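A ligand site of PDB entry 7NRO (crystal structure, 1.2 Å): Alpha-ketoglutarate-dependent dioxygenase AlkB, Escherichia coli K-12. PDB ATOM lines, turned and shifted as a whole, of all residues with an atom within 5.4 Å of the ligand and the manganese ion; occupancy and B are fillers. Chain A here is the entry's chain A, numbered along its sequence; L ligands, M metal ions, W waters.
OH of Tyr 122 sits at hydrogen-bond distance from O6 of the ligand, 2.8 Å away.
ND2 of Asn 120 sits at hydrogen-bond distance from O2 of the ligand.
NH1 of Arg 204 lies within salt-bridge range of O6 of the ligand (2.8 Å).
An oxygen (O3) of the ligand is in hydrogen-bond range of the side-chain hydroxyl (OH) of Tyr 76.
OD1 of Asn 206 sits close to O1 of the ligand.
Residues that only touch the ligand: Leu 118, Leu 128, Ile 189, Trp 69, Met 61, Arg 210, Gln 132, Phe 154 and Leu 170.
Hydrophobic or aromatic side chains within 4 Å of the ligand: Met 61, Trp 69, Tyr 76, Leu 118, Tyr 122, Leu 128, His 131, Phe 154, Leu 170, His 187 and Ile 189.
17 residues have an atom within 4 Å of the ligand: Met 61, Trp 69, Tyr 76, Leu 118, Asn 120, Tyr 122, Leu 128, His 131, Gln 132, Asp 133, Phe 154, Leu 170, His 187, Ile 189, Arg 204, Asn 206 and Arg 210.
Along chain A the residues within 4 Å of the ligand span positions 61 to 210.
The nearest printed residue that does not touch the ligand is Ser 145 (4.1 Å).
The nearest printed residue that does not touch the manganese ion is Arg 210 (4.5 Å).
Water W1 bridges the guanidinium group (NH2) of Arg 210 (3.4 Å) and the side-chain carboxylate (OD2) of Asp 133 (3.4 Å).
Water W2 lies within hydrogen-bond range of an oxygen (O2) of the ligand (2.7 Å), the side-chain hydroxyl (OG1) of Thr 208 (2.7 Å), the backbone carbonyl oxygen (O) of Asn 206 (2.9 Å) and the backbone carbonyl oxygen (O) of Leu 118 (3.3 Å).
Water W3 lies within hydrogen-bond range of OG of Ser 145 and O1 of the ligand.
Water W4 bridges the backbone carbonyl oxygen of Gln 132 (2.8 Å) and an oxygen (O4) of the ligand (3.1 Å).
OD1 of Asp 133 binds the manganese ion, at 2.1 Å.
O5 of the ligand is bound to the manganese ion, 2.2 Å away.
NE2 of His 187 is bound to the manganese ion, 2.2 Å away.
The manganese ion is bound by a ring nitrogen (NE2) of His 131, at 2.2 Å.
The manganese ion is bound by a nitrogen (N1) of the ligand, 2.2 Å away.
The manganese ion is bound by water W1, 2.4 Å away.
The manganese ion has six donor atoms within binding distance.
OD2 of Asp 133 is in salt-bridge range of NH1 of Arg 210, at 2.9 Å.
N of Tyr 122 is in hydrogen-bond range of O of Arg 204 (2.8 Å).
O of Asn 120 sits at hydrogen-bond distance from N of Asn 206 (2.8 Å).
NH2 of Arg 204 is in hydrogen-bond range of OD1 of Asn 206 (3.2 Å).
The side-chain amide oxygen of Asn 206 lies within hydrogen-bond range of the side-chain hydroxyl of Ser 145 (3.1 Å).
OG of Ser 147 lies within hydrogen-bond range of OD1 of Asn 206, at 3.4 Å.
The backbone carbonyl oxygen (O) of Leu 118 is in hydrogen-bond range of the backbone NH (N) of Thr 208, at 2.9 Å.
O of Ile 189 sits at hydrogen-bond distance from N of Leu 128, at 3.0 Å.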
ATOM      1  N   THR A  51     -16.914 -15.128  15.164  1.00  0.00           N
ATOM      2  CA  THR A  51     -16.837 -15.193  13.727  1.00  0.00           C
ATOM      3  C   THR A  51     -17.724 -16.316  13.207  1.00  0.00           C
ATOM      4  O   THR A  51     -18.204 -17.162  13.965  1.00  0.00           O
ATOM      5  CB  THR A  51     -15.414 -15.495  13.267  1.00  0.00           C
ATOM      6  OG1 THR A  51     -15.085 -16.843  13.666  1.00  0.00           O
ATOM      7  CG2 THR A  51     -14.438 -14.572  13.879  1.00  0.00           C
ATOM      8  N   MET A  57     -13.521 -13.203  18.507  1.00  0.00           N
ATOM      9  CA  MET A  57     -12.499 -12.270  18.083  1.00  0.00           C
ATOM     10  C   MET A  57     -11.799 -11.683  19.294  1.00  0.00           C
ATOM     11  O   MET A  57     -12.388 -11.461  20.349  1.00  0.00           O
ATOM     12  CB  MET A  57     -13.154 -11.163  17.269  1.00  0.00           C
ATOM     13  CG  MET A  57     -13.775 -11.650  15.992  1.00  0.00           C
ATOM     14  SD  MET A  57     -14.607 -10.324  15.106  1.00  0.00           S
ATOM     15  CE  MET A  57     -13.273  -9.579  14.223  1.00  0.00           C
ATOM     16  N   MET A  61     -15.834  -4.713  19.697  1.00  0.00           N
ATOM     17  CA  MET A  61     -16.401  -3.733  18.792  1.00  0.00           C
ATOM     18  C   MET A  61     -17.751  -3.225  19.271  1.00  0.00           C
ATOM     19  O   MET A  61     -18.432  -3.854  20.076  1.00  0.00           O
ATOM     20  CB  MET A  61     -16.570  -4.352  17.409  1.00  0.00           C
ATOM     21  CG  MET A  61     -15.265  -4.753  16.762  1.00  0.00           C
ATOM     22  SD  MET A  61     -15.542  -5.251  15.033  1.00  0.00           S
ATOM     23  CE  MET A  61     -14.076  -6.243  14.761  1.00  0.00           C
ATOM     24  N   TRP A  69     -22.141  -2.725  11.861  1.00  0.00           N
ATOM     25  CA  TRP A  69     -21.611  -3.994  11.384  1.00  0.00           C
ATOM     26  C   TRP A  69     -21.624  -5.002  12.512  1.00  0.00           C
ATOM     27  O   TRP A  69     -21.178  -4.710  13.616  1.00  0.00           O
ATOM     28  CB  TRP A  69     -20.198  -3.743  10.890  1.00  0.00           C
ATOM     29  CG  TRP A  69     -19.550  -4.868  10.214  1.00  0.00           C
ATOM     30  CD1 TRP A  69     -19.630  -5.157   8.876  1.00  0.00           C
ATOM     31  CD2 TRP A  69     -18.687  -5.837  10.803  1.00  0.00           C
ATOM     32  NE1 TRP A  69     -18.854  -6.271   8.589  1.00  0.00           N
ATOM     33  CE2 TRP A  69     -18.237  -6.682   9.746  1.00  0.00           C
ATOM     34  CE3 TRP A  69     -18.220  -6.073  12.085  1.00  0.00           C
ATOM     35  CZ2 TRP A  69     -17.372  -7.762   9.958  1.00  0.00           C
ATOM     36  CZ3 TRP A  69     -17.335  -7.148  12.291  1.00  0.00           C
ATOM     37  CH2 TRP A  69     -16.926  -7.964  11.228  1.00  0.00           C
ATOM     38  N   TYR A  76     -21.945 -11.971   8.505  1.00  0.00           N
ATOM     39  CA  TYR A  76     -21.692 -10.564   8.797  1.00  0.00           C
ATOM     40  C   TYR A  76     -22.693  -9.731   8.009  1.00  0.00           C
ATOM     41  O   TYR A  76     -23.012 -10.055   6.862  1.00  0.00           O
ATOM     42  CB  TYR A  76     -20.287 -10.153   8.385  1.00  0.00           C
ATOM     43  CG  TYR A  76     -19.198 -10.827   9.178  1.00  0.00           C
ATOM     44  CD1 TYR A  76     -19.094 -10.633  10.547  1.00  0.00           C
ATOM     45  CD2 TYR A  76     -18.245 -11.649   8.562  1.00  0.00           C
ATOM     46  CE1 TYR A  76     -18.107 -11.247  11.297  1.00  0.00           C
ATOM     47  CE2 TYR A  76     -17.231 -12.253   9.302  1.00  0.00           C
ATOM     48  CZ  TYR A  76     -17.174 -12.036  10.670  1.00  0.00           C
ATOM     49  OH  TYR A  76     -16.198 -12.640  11.440  1.00  0.00           O
ATOM     50  N   LEU A 118     -17.958   1.675  12.640  1.00  0.00           N
ATOM     51  CA  LEU A 118     -17.557   0.572  13.482  1.00  0.00           C
ATOM     52  C   LEU A 118     -16.405   1.043  14.351  1.00  0.00           C
ATOM     53  O   LEU A 118     -15.401   1.594  13.860  1.00  0.00           O
ATOM     54  CB  LEU A 118     -17.111  -0.561  12.579  1.00  0.00           C
ATOM     55  CG  LEU A 118     -16.759  -1.868  13.282  1.00  0.00           C
ATOM     56  CD1 LEU A 118     -17.792  -2.498  14.137  1.00  0.00           C
ATOM     57  CD2 LEU A 118     -16.338  -2.893  12.196  1.00  0.00           C
ATOM     58  N   ASN A 120     -13.608  -0.167  16.957  1.00  0.00           N
ATOM     59  CA  ASN A 120     -12.862  -1.376  17.269  1.00  0.00           C
ATOM     60  C   ASN A 120     -11.819  -1.072  18.323  1.00  0.00           C
ATOM     61  O   ASN A 120     -10.923  -0.276  18.095  1.00  0.00           O
ATOM     62  CB  ASN A 120     -12.232  -1.877  15.958  1.00  0.00           C
ATOM     63  CG  ASN A 120     -11.497  -3.182  16.127  1.00  0.00           C
ATOM     64  OD1 ASN A 120     -11.276  -3.631  17.259  1.00  0.00           O
ATOM     65  ND2 ASN A 120     -11.027  -3.760  15.035  1.00  0.00           N
ATOM     66  N   TYR A 122      -8.739  -2.505  20.539  1.00  0.00           N
ATOM     67  CA  TYR A 122      -7.655  -3.493  20.626  1.00  0.00           C
ATOM     68  C   TYR A 122      -7.025  -3.372  21.993  1.00  0.00           C
ATOM     69  O   TYR A 122      -6.429  -2.359  22.332  1.00  0.00           O
ATOM     70  CB  TYR A 122      -6.590  -3.203  19.583  1.00  0.00           C
ATOM     71  CG  TYR A 122      -6.978  -3.345  18.166  1.00  0.00           C
ATOM     72  CD1 TYR A 122      -7.764  -2.363  17.509  1.00  0.00           C
ATOM     73  CD2 TYR A 122      -6.576  -4.447  17.416  1.00  0.00           C
ATOM     74  CE1 TYR A 122      -8.104  -2.484  16.151  1.00  0.00           C
ATOM     75  CE2 TYR A 122      -6.904  -4.561  16.087  1.00  0.00           C
ATOM     76  CZ  TYR A 122      -7.666  -3.604  15.461  1.00  0.00           C
ATOM     77  OH  TYR A 122      -8.002  -3.787  14.122  1.00  0.00           O
ATOM     78  N   LEU A 128      -6.344  -8.447  14.112  1.00  0.00           N
ATOM     79  CA  LEU A 128      -7.368  -8.715  13.116  1.00  0.00           C
ATOM     80  C   LEU A 128      -6.703  -9.446  11.980  1.00  0.00           C
ATOM     81  O   LEU A 128      -5.809  -8.876  11.332  1.00  0.00           O
ATOM     82  CB  LEU A 128      -7.898  -7.409  12.563  1.00  0.00           C
ATOM     83  CG  LEU A 128      -9.313  -6.979  12.946  1.00  0.00           C
ATOM     84  CD1 LEU A 128      -9.687  -5.818  11.968  1.00  0.00           C
ATOM     85  CD2 LEU A 128     -10.341  -8.090  12.983  1.00  0.00           C
ATOM     86  N   HIS A 131      -8.137  -9.894   5.888  1.00  0.00           N
ATOM     87  CA  HIS A 131      -9.506  -9.961   5.408  1.00  0.00           C
ATOM     88  C   HIS A 131      -9.710  -8.844   4.394  1.00  0.00           C
ATOM     89  O   HIS A 131      -8.928  -7.915   4.271  1.00  0.00           O
ATOM     90  CB  HIS A 131     -10.528  -9.798   6.535  1.00  0.00           C
ATOM     91  CG  HIS A 131     -10.464  -8.447   7.167  1.00  0.00           C
ATOM     92  ND1 HIS A 131      -9.514  -8.109   8.110  1.00  0.00           N
ATOM     93  CD2 HIS A 131     -11.159  -7.329   6.913  1.00  0.00           C
ATOM     94  CE1 HIS A 131      -9.667  -6.837   8.418  1.00  0.00           C
ATOM     95  NE2 HIS A 131     -10.665  -6.347   7.720  1.00  0.00           N
ATOM     96  N   GLN A 132     -10.842  -8.918   3.686  1.00  0.00           N
ATOM     97  CA  GLN A 132     -11.382  -7.827   2.879  1.00  0.00           C
ATOM     98  C   GLN A 132     -12.657  -7.315   3.511  1.00  0.00           C
ATOM     99  O   GLN A 132     -13.391  -8.060   4.146  1.00  0.00           O
ATOM    100  CB  GLN A 132     -11.672  -8.303   1.461  1.00  0.00           C
ATOM    101  CG  GLN A 132     -10.462  -8.612   0.617  1.00  0.00           C
ATOM    102  CD  GLN A 132     -10.856  -9.143  -0.741  1.00  0.00           C
ATOM    103  OE1 GLN A 132     -10.544  -8.542  -1.774  1.00  0.00           O
ATOM    104  NE2 GLN A 132     -11.581 -10.242  -0.750  1.00  0.00           N
ATOM    105  N   ASP A 133     -12.967  -6.040   3.281  1.00  0.00           N
ATOM    106  CA  ASP A 133     -14.258  -5.469   3.636  1.00  0.00           C
ATOM    107  C   ASP A 133     -15.056  -5.387   2.351  1.00  0.00           C
ATOM    108  O   ASP A 133     -14.849  -4.486   1.520  1.00  0.00           O
ATOM    109  CB  ASP A 133     -14.046  -4.082   4.232  1.00  0.00           C
ATOM    110  CG  ASP A 133     -13.631  -4.114   5.650  1.00  0.00           C
ATOM    111  OD1 ASP A 133     -12.464  -4.367   5.911  1.00  0.00           O
ATOM    112  OD2 ASP A 133     -14.489  -3.948   6.538  1.00  0.00           O
ATOM    113  N   ASP A 135     -18.675  -6.133   2.477  1.00  0.00           N
ATOM    114  CA  ASP A 135     -20.073  -6.250   2.890  1.00  0.00           C
ATOM    115  C   ASP A 135     -20.902  -5.019   2.539  1.00  0.00           C
ATOM    116  O   ASP A 135     -22.114  -5.017   2.786  1.00  0.00           O
ATOM    117  CB  ASP A 135     -20.140  -6.451   4.412  1.00  0.00           C
ATOM    118  CG  ASP A 135     -19.504  -7.742   4.856  1.00  0.00           C
ATOM    119  OD1 ASP A 135     -19.843  -8.796   4.257  1.00  0.00           O
ATOM    120  OD2 ASP A 135     -18.670  -7.707   5.791  1.00  0.00           O
ATOM    121  N   SER A 145     -10.665   5.426   7.996  1.00  0.00           N
ATOM    122  CA  SER A 145     -10.173   4.676   9.153  1.00  0.00           C
ATOM    123  C   SER A 145      -9.308   5.547  10.053  1.00  0.00           C
ATOM    124  O   SER A 145      -8.229   5.950   9.631  1.00  0.00           O
ATOM    125  CB  SER A 145      -9.266   3.534   8.672  1.00  0.00           C
ATOM    126  OG  SER A 145      -8.499   3.086   9.794  1.00  0.00           O
ATOM    127  N   SER A 147      -7.235   6.054  13.645  1.00  0.00           N
ATOM    128  CA  SER A 147      -6.519   5.384  14.717  1.00  0.00           C
ATOM    129  C   SER A 147      -6.366   6.278  15.922  1.00  0.00           C
ATOM    130  O   SER A 147      -6.031   7.464  15.774  1.00  0.00           O
ATOM    131  CB  SER A 147      -5.107   5.055  14.250  1.00  0.00           C
ATOM    132  OG  SER A 147      -5.058   4.049  13.254  1.00  0.00           O
ATOM    133  N   PHE A 154      -0.315  -2.147  10.661  1.00  0.00           N
ATOM    134  CA  PHE A 154      -1.302  -2.479   9.666  1.00  0.00           C
ATOM    135  C   PHE A 154      -0.633  -3.136   8.471  1.00  0.00           C
ATOM    136  O   PHE A 154       0.365  -2.635   7.926  1.00  0.00           O
ATOM    137  CB  PHE A 154      -1.943  -1.176   9.229  1.00  0.00           C
ATOM    138  CG  PHE A 154      -3.061  -1.342   8.212  1.00  0.00           C
ATOM    139  CD1 PHE A 154      -4.352  -1.549   8.592  1.00  0.00           C
ATOM    140  CD2 PHE A 154      -2.805  -1.272   6.876  1.00  0.00           C
ATOM    141  CE1 PHE A 154      -5.387  -1.667   7.659  1.00  0.00           C
ATOM    142  CE2 PHE A 154      -3.847  -1.383   5.941  1.00  0.00           C
ATOM    143  CZ  PHE A 154      -5.125  -1.596   6.355  1.00  0.00           C
ATOM    144  N   LEU A 170       0.458   2.559  12.204  1.00  0.00           N
ATOM    145  CA  LEU A 170      -0.581   3.548  12.357  1.00  0.00           C
ATOM    146  C   LEU A 170      -0.562   4.019  13.788  1.00  0.00           C
ATOM    147  O   LEU A 170      -0.624   3.191  14.724  1.00  0.00           O
ATOM    148  CB  LEU A 170      -1.939   2.976  12.023  1.00  0.00           C
ATOM    149  CG  LEU A 170      -2.108   2.529  10.588  1.00  0.00           C
ATOM    150  CD1 LEU A 170      -3.475   1.933  10.347  1.00  0.00           C
ATOM    151  CD2 LEU A 170      -1.849   3.668   9.617  1.00  0.00           C
ATOM    152  N   HIS A 187      -6.255  -6.930   4.164  1.00  0.00           N
ATOM    153  CA  HIS A 187      -5.541  -6.162   5.169  1.00  0.00           C
ATOM    154  C   HIS A 187      -5.829  -6.755   6.533  1.00  0.00           C
ATOM    155  O   HIS A 187      -6.786  -7.534   6.731  1.00  0.00           O
ATOM    156  CB  HIS A 187      -5.920  -4.667   5.093  1.00  0.00           C
ATOM    157  CG  HIS A 187      -7.388  -4.449   5.320  1.00  0.00           C
ATOM    158  ND1 HIS A 187      -8.328  -4.605   4.330  1.00  0.00           N
ATOM    159  CD2 HIS A 187      -8.087  -4.117   6.433  1.00  0.00           C
ATOM    160  CE1 HIS A 187      -9.546  -4.442   4.851  1.00  0.00           C
ATOM    161  NE2 HIS A 187      -9.421  -4.088   6.114  1.00  0.00           N
ATOM    162  N   ILE A 189      -4.382  -6.274  11.096  1.00  0.00           N
ATOM    163  CA  ILE A 189      -3.628  -5.598  12.138  1.00  0.00           C
ATOM    164  C   ILE A 189      -2.929  -6.679  12.941  1.00  0.00           C
ATOM    165  O   ILE A 189      -3.571  -7.648  13.385  1.00  0.00           O
ATOM    166  CB  ILE A 189      -4.557  -4.767  13.039  1.00  0.00           C
ATOM    167  CG1 ILE A 189      -5.066  -3.529  12.289  1.00  0.00           C
ATOM    168  CG2 ILE A 189      -3.836  -4.394  14.330  1.00  0.00           C
ATOM    169  CD1 ILE A 189      -4.078  -2.423  12.320  1.00  0.00           C
ATOM    170  N   ARG A 204      -5.818   0.579  21.869  1.00  0.00           N
ATOM    171  CA  ARG A 204      -5.994   1.297  20.629  1.00  0.00           C
ATOM    172  C   ARG A 204      -7.459   1.242  20.264  1.00  0.00           C
ATOM    173  O   ARG A 204      -8.110   0.192  20.420  1.00  0.00           O
ATOM    174  CB  ARG A 204      -5.188   0.645  19.527  1.00  0.00           C
ATOM    175  CG  ARG A 204      -5.417   1.234  18.168  1.00  0.00           C
ATOM    176  CD  ARG A 204      -4.538   0.544  17.139  1.00  0.00           C
ATOM    177  NE  ARG A 204      -4.639   1.117  15.784  1.00  0.00           N
ATOM    178  CZ  ARG A 204      -5.298   0.581  14.755  1.00  0.00           C
ATOM    179  NH1 ARG A 204      -5.909  -0.584  14.824  1.00  0.00           N
ATOM    180  NH2 ARG A 204      -5.297   1.226  13.594  1.00  0.00           N
ATOM    181  N   ASN A 206      -9.854   1.928  16.735  1.00  0.00           N
ATOM    182  CA  ASN A 206      -9.901   2.312  15.338  1.00  0.00           C
ATOM    183  C   ASN A 206     -11.355   2.502  14.940  1.00  0.00           C
ATOM    184  O   ASN A 206     -12.202   1.611  15.171  1.00  0.00           O
ATOM    185  CB  ASN A 206      -9.316   1.237  14.458  1.00  0.00           C
ATOM    186  CG  ASN A 206      -9.057   1.745  13.051  1.00  0.00           C
ATOM    187  OD1 ASN A 206      -8.099   2.491  12.835  1.00  0.00           O
ATOM    188  ND2 ASN A 206      -9.889   1.402  12.132  1.00  0.00           N
ATOM    189  N   THR A 208     -13.894   2.894  11.768  1.00  0.00           N
ATOM    190  CA  THR A 208     -14.014   2.748  10.321  1.00  0.00           C
ATOM    191  C   THR A 208     -15.410   3.191   9.910  1.00  0.00           C
ATOM    192  O   THR A 208     -16.437   2.571  10.248  1.00  0.00           O
ATOM    193  CB  THR A 208     -13.734   1.339   9.806  1.00  0.00           C
ATOM    194  OG1 THR A 208     -14.317   0.317  10.605  1.00  0.00           O
ATOM    195  CG2 THR A 208     -12.239   1.092   9.679  1.00  0.00           C
ATOM    196  N   ARG A 210     -18.253   3.852   7.155  1.00  0.00           N
ATOM    197  CA  ARG A 210     -18.709   3.106   5.996  1.00  0.00           C
ATOM    198  C   ARG A 210     -20.042   3.645   5.513  1.00  0.00           C
ATOM    199  O   ARG A 210     -20.895   4.077   6.314  1.00  0.00           O
ATOM    200  CB  ARG A 210     -18.927   1.631   6.377  1.00  0.00           C
ATOM    201  CG  ARG A 210     -17.684   0.925   6.984  1.00  0.00           C
ATOM    202  CD  ARG A 210     -17.911   0.183   8.320  1.00  0.00           C
ATOM    203  NE  ARG A 210     -16.679  -0.428   8.848  1.00  0.00           N
ATOM    204  CZ  ARG A 210     -16.021  -1.423   8.242  1.00  0.00           C
ATOM    205  NH1 ARG A 210     -16.586  -2.145   7.287  1.00  0.00           N
ATOM    206  NH2 ARG A 210     -14.750  -1.693   8.582  1.00  0.00           N
HETATM  207  N1  LIG L   1     -12.136  -4.141   9.502  1.00  0.00           N
HETATM  208  C1  LIG L   1     -14.592  -8.954   7.562  1.00  0.00           C
HETATM  209  C2  LIG L   1     -14.059  -9.717   8.582  1.00  0.00           C
HETATM  210  N2  LIG L   1     -13.627  -5.701   8.926  1.00  0.00           N
HETATM  211  C3  LIG L   1     -13.452  -9.156   9.677  1.00  0.00           C
HETATM  212  O1  LIG L   1      -6.594  -0.153  11.446  1.00  0.00           O
HETATM  213  C4  LIG L   1      -8.385  -1.339  10.564  1.00  0.00           C
HETATM  214  O2  LIG L   1     -11.425  -2.363  12.616  1.00  0.00           O
HETATM  215  C5  LIG L   1     -13.955  -6.984   8.768  1.00  0.00           C
HETATM  216  C6  LIG L   1     -14.531  -7.577   7.660  1.00  0.00           C
HETATM  217  N3  LIG L   1     -14.202 -11.178   8.520  1.00  0.00           N
HETATM  218  C7  LIG L   1     -13.187  -4.858   9.881  1.00  0.00           C
HETATM  219  O3  LIG L   1     -13.775 -11.845   9.446  1.00  0.00           O
HETATM  220  C8  LIG L   1     -11.526  -3.355  10.428  1.00  0.00           C
HETATM  221  O4  LIG L   1     -14.782 -11.661   7.551  1.00  0.00           O
HETATM  222  C9  LIG L   1      -7.526  -0.907  11.740  1.00  0.00           C
HETATM  223  N4  LIG L   1      -9.628  -2.002  10.887  1.00  0.00           N
HETATM  224  C10 LIG L   1     -10.259  -2.772   9.992  1.00  0.00           C
HETATM  225  O5  LIG L   1      -9.843  -3.015   8.857  1.00  0.00           O
HETATM  226  C11 LIG L   1     -13.412  -7.771   9.775  1.00  0.00           C
HETATM  227  C12 LIG L   1     -13.727  -4.792  11.163  1.00  0.00           C
HETATM  228  C13 LIG L   1     -13.150  -3.929  12.068  1.00  0.00           C
HETATM  229  C14 LIG L   1     -12.019  -3.196  11.722  1.00  0.00           C
HETATM  230  O6  LIG L   1      -7.840  -1.310  12.867  1.00  0.00           O
HETATM  231 MN    MN M   1     -11.107  -4.155   7.503  1.00  0.00          MN
HETATM  232  O   HOH W   1     -11.801  -1.911   6.984  1.00  0.00           O
HETATM  233  O   HOH W   2     -12.769  -0.084  12.826  1.00  0.00           O
HETATM  234  O   HOH W   3      -6.712   1.519   9.173  1.00  0.00           O
HETATM  235  O   HOH W   4     -14.583 -10.548   4.617  1.00  0.00           O
HETATM  236  O   HOH W   5      -9.223  -0.593   7.162  1.00  0.00           O
